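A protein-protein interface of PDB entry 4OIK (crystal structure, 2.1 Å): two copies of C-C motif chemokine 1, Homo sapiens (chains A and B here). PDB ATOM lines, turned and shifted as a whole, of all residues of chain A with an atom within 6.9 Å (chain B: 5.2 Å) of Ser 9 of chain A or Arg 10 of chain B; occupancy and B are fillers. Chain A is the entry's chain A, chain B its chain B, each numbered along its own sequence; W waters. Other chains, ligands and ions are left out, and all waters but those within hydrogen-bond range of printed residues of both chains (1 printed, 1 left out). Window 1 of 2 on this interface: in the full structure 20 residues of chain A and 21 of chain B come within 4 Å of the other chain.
Cys 11 of chain B touches Phe 8 of chain A (O to CA, 3.3 Å). Phe 8 of chain A touches Ile 41 of chain B. CD2 of Phe 13 of chain B touches OG of Ser 9 of chain A, at 3.5 Å. CD of Arg 10 of chain A touches CE1 of Phe 8 of chain B, 3.5 Å away. Ser 9 of chain B touches Arg 10 of chain A (O to CA, 3.6 Å). CA of Phe 8 of chain B touches O of Cys 11 of chain A, at 3.3 Å. Cys 11 of chain A touches Phe 13 of chain B. Ser 9 of chain B touches Phe 13 of chain A (OG to CD2, 3.5 Å). Phe 13 of chain A touches Cys 11 of chain B (CE2 to SG, 3.8 Å). Cys 35 of chain A touches Phe 13 of chain B.
OG of Ser 32 of chain A is in hydrogen-bond range of N of Arg 10 of chain A (2.8 Å). The side-chain sulfur of Cys 35 of chain A is disulfide-bonded to the side-chain sulfur of Cys 11 of chain A, 2.0 Å away. N of Arg 10 of chain B sits at hydrogen-bond distance from OG of Ser 32 of chain B, 2.8 Å away. SG of Cys 35 of chain B is disulfide-bonded to SG of Cys 11 of chain B, 2.0 Å away. The backbone NH (N) of Arg 29 of chain B lies within hydrogen-bond range of the backbone carbonyl oxygen (O) of Ile 41 of chain B (2.6 Å).
Printed residues of chain B that touch a printed residue of chain A: Phe 8, Ser 9, Arg 10, Cys 11, Phe 13 and Ile 41. Among the printed residues, 17 pairs touch across the chains.
The backbone NH (N) of Ser 9 of chain A sits at hydrogen-bond distance from the backbone carbonyl oxygen (O) of Cys 11 of chain B (2.7 Å). The backbone carbonyl oxygen (O) of Cys 11 of chain A lies within hydrogen-bond range of the backbone NH (N) of Ser 9 of chain B, at 2.7 Å. O of Ser 9 of chain B sits close to O of Ser 9 of chain A, at 3.3 Å. The side-chain sulfur (SG) of Cys 11 of chain A sits close to the side-chain sulfur (SG) of Cys 11 of chain B (3.7 Å).
Phe 8 of chain A touches Arg 10 of chain B, and with the chains exchanged Arg 10 of chain A touches Phe 8 of chain B. Phe 8 of chain A touches Cys 11 of chain B, and with the chains exchanged Cys 11 of chain A touches Phe 8 of chain B. Ser 9 of chain B touches its own counterpart, Ser 9 of chain A. Ser 9 of chain A touches Arg 10 of chain B, and with the chains exchanged Arg 10 of chain A touches Ser 9 of chain B. 8 positions are printed for both chains. Of the 17 pairs that touch across the chains among the printed residues, 14 have their exchanged pair printed and touching as well.
Water W1 lies within hydrogen-bond range of OG of Ser 9 of chain B and N of Phe 13 of chain A.
Of chain B, only Ser 9, Arg 10, Cys 11 and Phe 13 come within 4 Å of Ser 9 of chain A. Of chain A, only Phe 8 (3.5 Å) and Ser 9 (3.7 Å) come within 4 Å of Arg 10 of chain B. Printed residues of chain B within 4 Å of Arg 10 of chain A: Phe 8 and Ser 9. Of the printed residues of chain A, Ile 41 of chain B touches Phe 8 (3.9 Å). Thr 31 of chain B touches none of the printed residues of chain A. The nearest residue of chain B that does not touch Ser 9 of chain A is Cys 12 of chain B (4.9 Å). The nearest printed residue of chain A that does not touch Arg 10 of chain B is Arg 10 of chain A (5.3 Å).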
ATOM      1  N   VAL A   6     -20.453 -23.791  -8.635  1.00  0.00           N
ATOM      2  CA  VAL A   6     -19.187 -23.359  -8.039  1.00  0.00           C
ATOM      3  C   VAL A   6     -19.137 -24.185  -6.728  1.00  0.00           C
ATOM      4  O   VAL A   6     -19.598 -23.768  -5.660  1.00  0.00           O
ATOM      5  CB  VAL A   6     -19.066 -21.811  -7.940  1.00  0.00           C
ATOM      6  CG1 VAL A   6     -20.398 -21.141  -7.619  1.00  0.00           C
ATOM      7  CG2 VAL A   6     -17.965 -21.370  -7.003  1.00  0.00           C
ATOM      8  N   PRO A   7     -18.747 -25.469  -6.890  1.00  0.00           N
ATOM      9  CA  PRO A   7     -18.801 -26.413  -5.785  1.00  0.00           C
ATOM     10  C   PRO A   7     -18.132 -25.999  -4.506  1.00  0.00           C
ATOM     11  O   PRO A   7     -17.216 -25.182  -4.508  1.00  0.00           O
ATOM     12  CB  PRO A   7     -18.141 -27.671  -6.358  1.00  0.00           C
ATOM     13  CG  PRO A   7     -17.384 -27.211  -7.519  1.00  0.00           C
ATOM     14  CD  PRO A   7     -18.244 -26.146  -8.099  1.00  0.00           C
ATOM     15  N   PHE A   8     -18.587 -26.581  -3.407  1.00  0.00           N
ATOM     16  CA  PHE A   8     -17.954 -26.327  -2.127  1.00  0.00           C
ATOM     17  C   PHE A   8     -16.736 -27.234  -2.107  1.00  0.00           C
ATOM     18  O   PHE A   8     -16.621 -28.151  -2.934  1.00  0.00           O
ATOM     19  CB  PHE A   8     -18.940 -26.604  -0.979  1.00  0.00           C
ATOM     20  CG  PHE A   8     -19.373 -28.051  -0.834  1.00  0.00           C
ATOM     21  CD1 PHE A   8     -18.646 -28.937  -0.046  1.00  0.00           C
ATOM     22  CD2 PHE A   8     -20.549 -28.499  -1.412  1.00  0.00           C
ATOM     23  CE1 PHE A   8     -19.053 -30.263   0.097  1.00  0.00           C
ATOM     24  CE2 PHE A   8     -20.965 -29.823  -1.255  1.00  0.00           C
ATOM     25  CZ  PHE A   8     -20.210 -30.690  -0.501  1.00  0.00           C
ATOM     26  N   SER A   9     -15.818 -26.961  -1.205  1.00  0.00           N
ATOM     27  CA  SER A   9     -14.604 -27.727  -1.053  1.00  0.00           C
ATOM     28  C   SER A   9     -14.796 -28.668   0.124  1.00  0.00           C
ATOM     29  O   SER A   9     -15.396 -28.272   1.142  1.00  0.00           O
ATOM     30  CB  SER A   9     -13.441 -26.786  -0.747  1.00  0.00           C
ATOM     31  OG  SER A   9     -13.366 -25.699  -1.660  1.00  0.00           O
ATOM     32  N   ARG A  10     -14.253 -29.886   0.027  1.00  0.00           N
ATOM     33  CA  ARG A  10     -14.303 -30.800   1.172  1.00  0.00           C
ATOM     34  C   ARG A  10     -12.963 -30.682   1.839  1.00  0.00           C
ATOM     35  O   ARG A  10     -11.946 -30.938   1.195  1.00  0.00           O
ATOM     36  CB  ARG A  10     -14.537 -32.251   0.736  1.00  0.00           C
ATOM     37  CG  ARG A  10     -15.859 -32.447   0.099  1.00  0.00           C
ATOM     38  CD  ARG A  10     -16.236 -33.899   0.064  1.00  0.00           C
ATOM     39  NE  ARG A  10     -17.532 -34.022  -0.596  1.00  0.00           N
ATOM     40  CZ  ARG A  10     -17.676 -34.250  -1.889  1.00  0.00           C
ATOM     41  NH1 ARG A  10     -18.886 -34.310  -2.423  1.00  0.00           N
ATOM     42  NH2 ARG A  10     -16.611 -34.412  -2.664  1.00  0.00           N
ATOM     43  N   CYS A  11     -12.948 -30.240   3.097  1.00  0.00           N
ATOM     44  CA  CYS A  11     -11.711 -30.021   3.854  1.00  0.00           C
ATOM     45  C   CYS A  11     -11.676 -30.815   5.114  1.00  0.00           C
ATOM     46  O   CYS A  11     -12.700 -31.061   5.745  1.00  0.00           O
ATOM     47  CB  CYS A  11     -11.526 -28.552   4.172  1.00  0.00           C
ATOM     48  SG  CYS A  11     -11.713 -27.466   2.752  1.00  0.00           S
ATOM     49  N   PHE A  13      -9.954 -30.313   8.671  1.00  0.00           N
ATOM     50  CA  PHE A  13      -9.214 -29.508   9.650  1.00  0.00           C
ATOM     51  C   PHE A  13      -8.984 -30.230  11.010  1.00  0.00           C
ATOM     52  O   PHE A  13      -8.178 -29.774  11.784  1.00  0.00           O
ATOM     53  CB  PHE A  13      -9.848 -28.137   9.851  1.00  0.00           C
ATOM     54  CG  PHE A  13      -9.988 -27.350   8.577  1.00  0.00           C
ATOM     55  CD1 PHE A  13      -8.873 -26.813   7.947  1.00  0.00           C
ATOM     56  CD2 PHE A  13     -11.238 -27.056   8.062  1.00  0.00           C
ATOM     57  CE1 PHE A  13      -8.999 -26.079   6.774  1.00  0.00           C
ATOM     58  CE2 PHE A  13     -11.363 -26.301   6.897  1.00  0.00           C
ATOM     59  CZ  PHE A  13     -10.241 -25.809   6.274  1.00  0.00           C
ATOM     60  N   THR A  31      -9.155 -34.734  -0.240  1.00  0.00           N
ATOM     61  CA  THR A  31      -9.757 -33.428   0.091  1.00  0.00           C
ATOM     62  C   THR A  31      -9.511 -32.462  -1.076  1.00  0.00           C
ATOM     63  O   THR A  31      -8.653 -32.719  -1.929  1.00  0.00           O
ATOM     64  CB  THR A  31      -9.181 -32.864   1.394  1.00  0.00           C
ATOM     65  OG1 THR A  31      -7.804 -32.597   1.195  1.00  0.00           O
ATOM     66  CG2 THR A  31      -9.350 -33.797   2.573  1.00  0.00           C
ATOM     67  N   SER A  32     -10.242 -31.350  -1.116  1.00  0.00           N
ATOM     68  CA  SER A  32     -10.067 -30.367  -2.186  1.00  0.00           C
ATOM     69  C   SER A  32      -8.670 -29.756  -2.133  1.00  0.00           C
ATOM     70  O   SER A  32      -8.162 -29.498  -1.042  1.00  0.00           O
ATOM     71  CB  SER A  32     -11.138 -29.296  -2.100  1.00  0.00           C
ATOM     72  OG  SER A  32     -12.408 -29.923  -2.108  1.00  0.00           O
ATOM     73  N   SER A  33      -8.047 -29.569  -3.314  1.00  0.00           N
ATOM     74  CA  SER A  33      -6.686 -29.056  -3.483  1.00  0.00           C
ATOM     75  C   SER A  33      -6.434 -27.681  -2.884  1.00  0.00           C
ATOM     76  O   SER A  33      -5.291 -27.344  -2.566  1.00  0.00           O
ATOM     77  CB  SER A  33      -6.290 -29.085  -4.948  1.00  0.00           C
ATOM     78  OG  SER A  33      -6.499 -30.395  -5.449  1.00  0.00           O
ATOM     79  N   ILE A  34      -7.493 -26.891  -2.716  1.00  0.00           N
ATOM     80  CA  ILE A  34      -7.394 -25.561  -2.132  1.00  0.00           C
ATOM     81  C   ILE A  34      -7.064 -25.611  -0.652  1.00  0.00           C
ATOM     82  O   ILE A  34      -6.341 -24.753  -0.178  1.00  0.00           O
ATOM     83  CB  ILE A  34      -8.652 -24.710  -2.459  1.00  0.00           C
ATOM     84  CG1 ILE A  34      -8.494 -23.228  -2.051  1.00  0.00           C
ATOM     85  CG2 ILE A  34      -9.965 -25.326  -1.964  1.00  0.00           C
ATOM     86  CD1 ILE A  34      -8.473 -22.337  -3.199  1.00  0.00           C
ATOM     87  N   CYS A  35      -7.581 -26.623   0.072  1.00  0.00           N
ATOM     88  CA  CYS A  35      -7.429 -26.781   1.516  1.00  0.00           C
ATOM     89  C   CYS A  35      -6.822 -28.139   1.843  1.00  0.00           C
ATOM     90  O   CYS A  35      -7.035 -28.626   2.960  1.00  0.00           O
ATOM     91  CB  CYS A  35      -8.796 -26.620   2.184  1.00  0.00           C
ATOM     92  SG  CYS A  35     -10.029 -27.860   1.664  1.00  0.00           S
ATOM     93  N   PHE B   8     -15.734 -34.196   7.508  1.00  0.00           N
ATOM     94  CA  PHE B   8     -15.024 -33.196   6.747  1.00  0.00           C
ATOM     95  C   PHE B   8     -15.856 -31.937   6.862  1.00  0.00           C
ATOM     96  O   PHE B   8     -17.017 -31.998   7.276  1.00  0.00           O
ATOM     97  CB  PHE B   8     -14.822 -33.657   5.300  1.00  0.00           C
ATOM     98  CG  PHE B   8     -16.090 -33.814   4.484  1.00  0.00           C
ATOM     99  CD1 PHE B   8     -16.625 -32.735   3.779  1.00  0.00           C
ATOM    100  CD2 PHE B   8     -16.703 -35.046   4.361  1.00  0.00           C
ATOM    101  CE1 PHE B   8     -17.779 -32.878   3.034  1.00  0.00           C
ATOM    102  CE2 PHE B   8     -17.859 -35.196   3.597  1.00  0.00           C
ATOM    103  CZ  PHE B   8     -18.389 -34.110   2.946  1.00  0.00           C
ATOM    104  N   SER B   9     -15.256 -30.801   6.553  1.00  0.00           N
ATOM    105  CA  SER B   9     -15.924 -29.515   6.616  1.00  0.00           C
ATOM    106  C   SER B   9     -16.366 -29.140   5.201  1.00  0.00           C
ATOM    107  O   SER B   9     -15.628 -29.382   4.245  1.00  0.00           O
ATOM    108  CB  SER B   9     -14.949 -28.457   7.128  1.00  0.00           C
ATOM    109  OG  SER B   9     -14.268 -28.866   8.307  1.00  0.00           O
ATOM    110  N   ARG B  10     -17.523 -28.503   5.064  1.00  0.00           N
ATOM    111  CA  ARG B  10     -17.946 -28.007   3.751  1.00  0.00           C
ATOM    112  C   ARG B  10     -17.598 -26.544   3.746  1.00  0.00           C
ATOM    113  O   ARG B  10     -18.096 -25.800   4.593  1.00  0.00           O
ATOM    114  CB  ARG B  10     -19.438 -28.177   3.518  1.00  0.00           C
ATOM    115  CG  ARG B  10     -19.818 -29.603   3.415  1.00  0.00           C
ATOM    116  CD  ARG B  10     -21.187 -29.798   2.831  1.00  0.00           C
ATOM    117  NE  ARG B  10     -21.499 -31.219   2.947  1.00  0.00           N
ATOM    118  CZ  ARG B  10     -22.219 -31.734   3.923  1.00  0.00           C
ATOM    119  NH1 ARG B  10     -22.807 -30.941   4.808  1.00  0.00           N
ATOM    120  NH2 ARG B  10     -22.408 -33.044   3.994  1.00  0.00           N
ATOM    121  N   CYS B  11     -16.714 -26.134   2.833  1.00  0.00           N
ATOM    122  CA  CYS B  11     -16.241 -24.752   2.751  1.00  0.00           C
ATOM    123  C   CYS B  11     -16.492 -24.163   1.413  1.00  0.00           C
ATOM    124  O   CYS B  11     -16.436 -24.858   0.401  1.00  0.00           O
ATOM    125  CB  CYS B  11     -14.760 -24.675   3.070  1.00  0.00           C
ATOM    126  SG  CYS B  11     -14.287 -25.500   4.595  1.00  0.00           S
ATOM    127  N   CYS B  12     -16.588 -22.847   1.406  1.00  0.00           N
ATOM    128  CA  CYS B  12     -16.772 -22.071   0.203  1.00  0.00           C
ATOM    129  C   CYS B  12     -15.669 -21.065   0.067  1.00  0.00           C
ATOM    130  O   CYS B  12     -15.697 -20.036   0.740  1.00  0.00           O
ATOM    131  CB  CYS B  12     -18.134 -21.411   0.237  1.00  0.00           C
ATOM    132  SG  CYS B  12     -19.463 -22.537  -0.199  1.00  0.00           S
ATOM    133  N   PHE B  13     -14.679 -21.373  -0.782  1.00  0.00           N
ATOM    134  CA  PHE B  13     -13.568 -20.451  -1.047  1.00  0.00           C
ATOM    135  C   PHE B  13     -13.716 -19.657  -2.385  1.00  0.00           C
ATOM    136  O   PHE B  13     -13.021 -18.678  -2.563  1.00  0.00           O
ATOM    137  CB  PHE B  13     -12.237 -21.167  -0.972  1.00  0.00           C
ATOM    138  CG  PHE B  13     -11.988 -21.852   0.347  1.00  0.00           C
ATOM    139  CD1 PHE B  13     -11.723 -21.112   1.498  1.00  0.00           C
ATOM    140  CD2 PHE B  13     -11.895 -23.228   0.417  1.00  0.00           C
ATOM    141  CE1 PHE B  13     -11.508 -21.743   2.715  1.00  0.00           C
ATOM    142  CE2 PHE B  13     -11.637 -23.863   1.631  1.00  0.00           C
ATOM    143  CZ  PHE B  13     -11.434 -23.113   2.768  1.00  0.00           C
ATOM    144  N   ARG B  29     -27.447 -25.001   2.259  1.00  0.00           N
ATOM    145  CA  ARG B  29     -26.654 -25.544   3.367  1.00  0.00           C
ATOM    146  C   ARG B  29     -25.761 -24.411   3.860  1.00  0.00           C
ATOM    147  O   ARG B  29     -25.278 -23.620   3.041  1.00  0.00           O
ATOM    148  CB  ARG B  29     -25.779 -26.733   2.936  1.00  0.00           C
ATOM    149  CG  ARG B  29     -26.436 -28.070   3.163  1.00  0.00           C
ATOM    150  CD  ARG B  29     -25.435 -29.177   3.404  1.00  0.00           C
ATOM    151  NE  ARG B  29     -25.980 -30.214   4.287  1.00  0.00           N
ATOM    152  CZ  ARG B  29     -25.937 -30.176   5.618  1.00  0.00           C
ATOM    153  NH1 ARG B  29     -25.389 -29.140   6.246  1.00  0.00           N
ATOM    154  NH2 ARG B  29     -26.446 -31.171   6.331  1.00  0.00           N
ATOM    155  N   THR B  31     -22.185 -23.223   5.510  1.00  0.00           N
ATOM    156  CA  THR B  31     -20.850 -23.833   5.465  1.00  0.00           C
ATOM    157  C   THR B  31     -20.408 -24.152   6.908  1.00  0.00           C
ATOM    158  O   THR B  31     -20.978 -23.616   7.868  1.00  0.00           O
ATOM    159  CB  THR B  31     -19.840 -22.906   4.787  1.00  0.00           C
ATOM    160  OG1 THR B  31     -19.694 -21.741   5.591  1.00  0.00           O
ATOM    161  CG2 THR B  31     -20.242 -22.517   3.388  1.00  0.00           C
ATOM    162  N   SER B  32     -19.395 -25.005   7.062  1.00  0.00           N
ATOM    163  CA  SER B  32     -18.896 -25.366   8.388  1.00  0.00           C
ATOM    164  C   SER B  32     -18.328 -24.124   9.096  1.00  0.00           C
ATOM    165  O   SER B  32     -17.675 -23.292   8.461  1.00  0.00           O
ATOM    166  CB  SER B  32     -17.847 -26.457   8.269  1.00  0.00           C
ATOM    167  OG  SER B  32     -18.397 -27.560   7.570  1.00  0.00           O
ATOM    168  N   CYS B  35     -14.610 -22.756   8.747  1.00  0.00           N
ATOM    169  CA  CYS B  35     -14.193 -22.076   7.525  1.00  0.00           C
ATOM    170  C   CYS B  35     -15.330 -21.211   6.995  1.00  0.00           C
ATOM    171  O   CYS B  35     -15.343 -20.936   5.794  1.00  0.00           O
ATOM    172  CB  CYS B  35     -13.779 -23.119   6.484  1.00  0.00           C
ATOM    173  SG  CYS B  35     -15.111 -24.288   6.019  1.00  0.00           S
ATOM    174  N   ILE B  41     -24.263 -22.338   0.738  1.00  0.00           N
ATOM    175  CA  ILE B  41     -24.253 -23.364  -0.312  1.00  0.00           C
ATOM    176  C   ILE B  41     -25.699 -23.568  -0.780  1.00  0.00           C
ATOM    177  O   ILE B  41     -26.542 -23.922   0.036  1.00  0.00           O
ATOM    178  CB  ILE B  41     -23.623 -24.727   0.136  1.00  0.00           C
ATOM    179  CG1 ILE B  41     -22.266 -24.543   0.811  1.00  0.00           C
ATOM    180  CG2 ILE B  41     -23.507 -25.692  -1.074  1.00  0.00           C
ATOM    181  CD1 ILE B  41     -21.786 -25.802   1.555  1.00  0.00           C
HETATM  182  O   HOH W   1     -12.559 -30.659   9.223  1.00  0.00           O
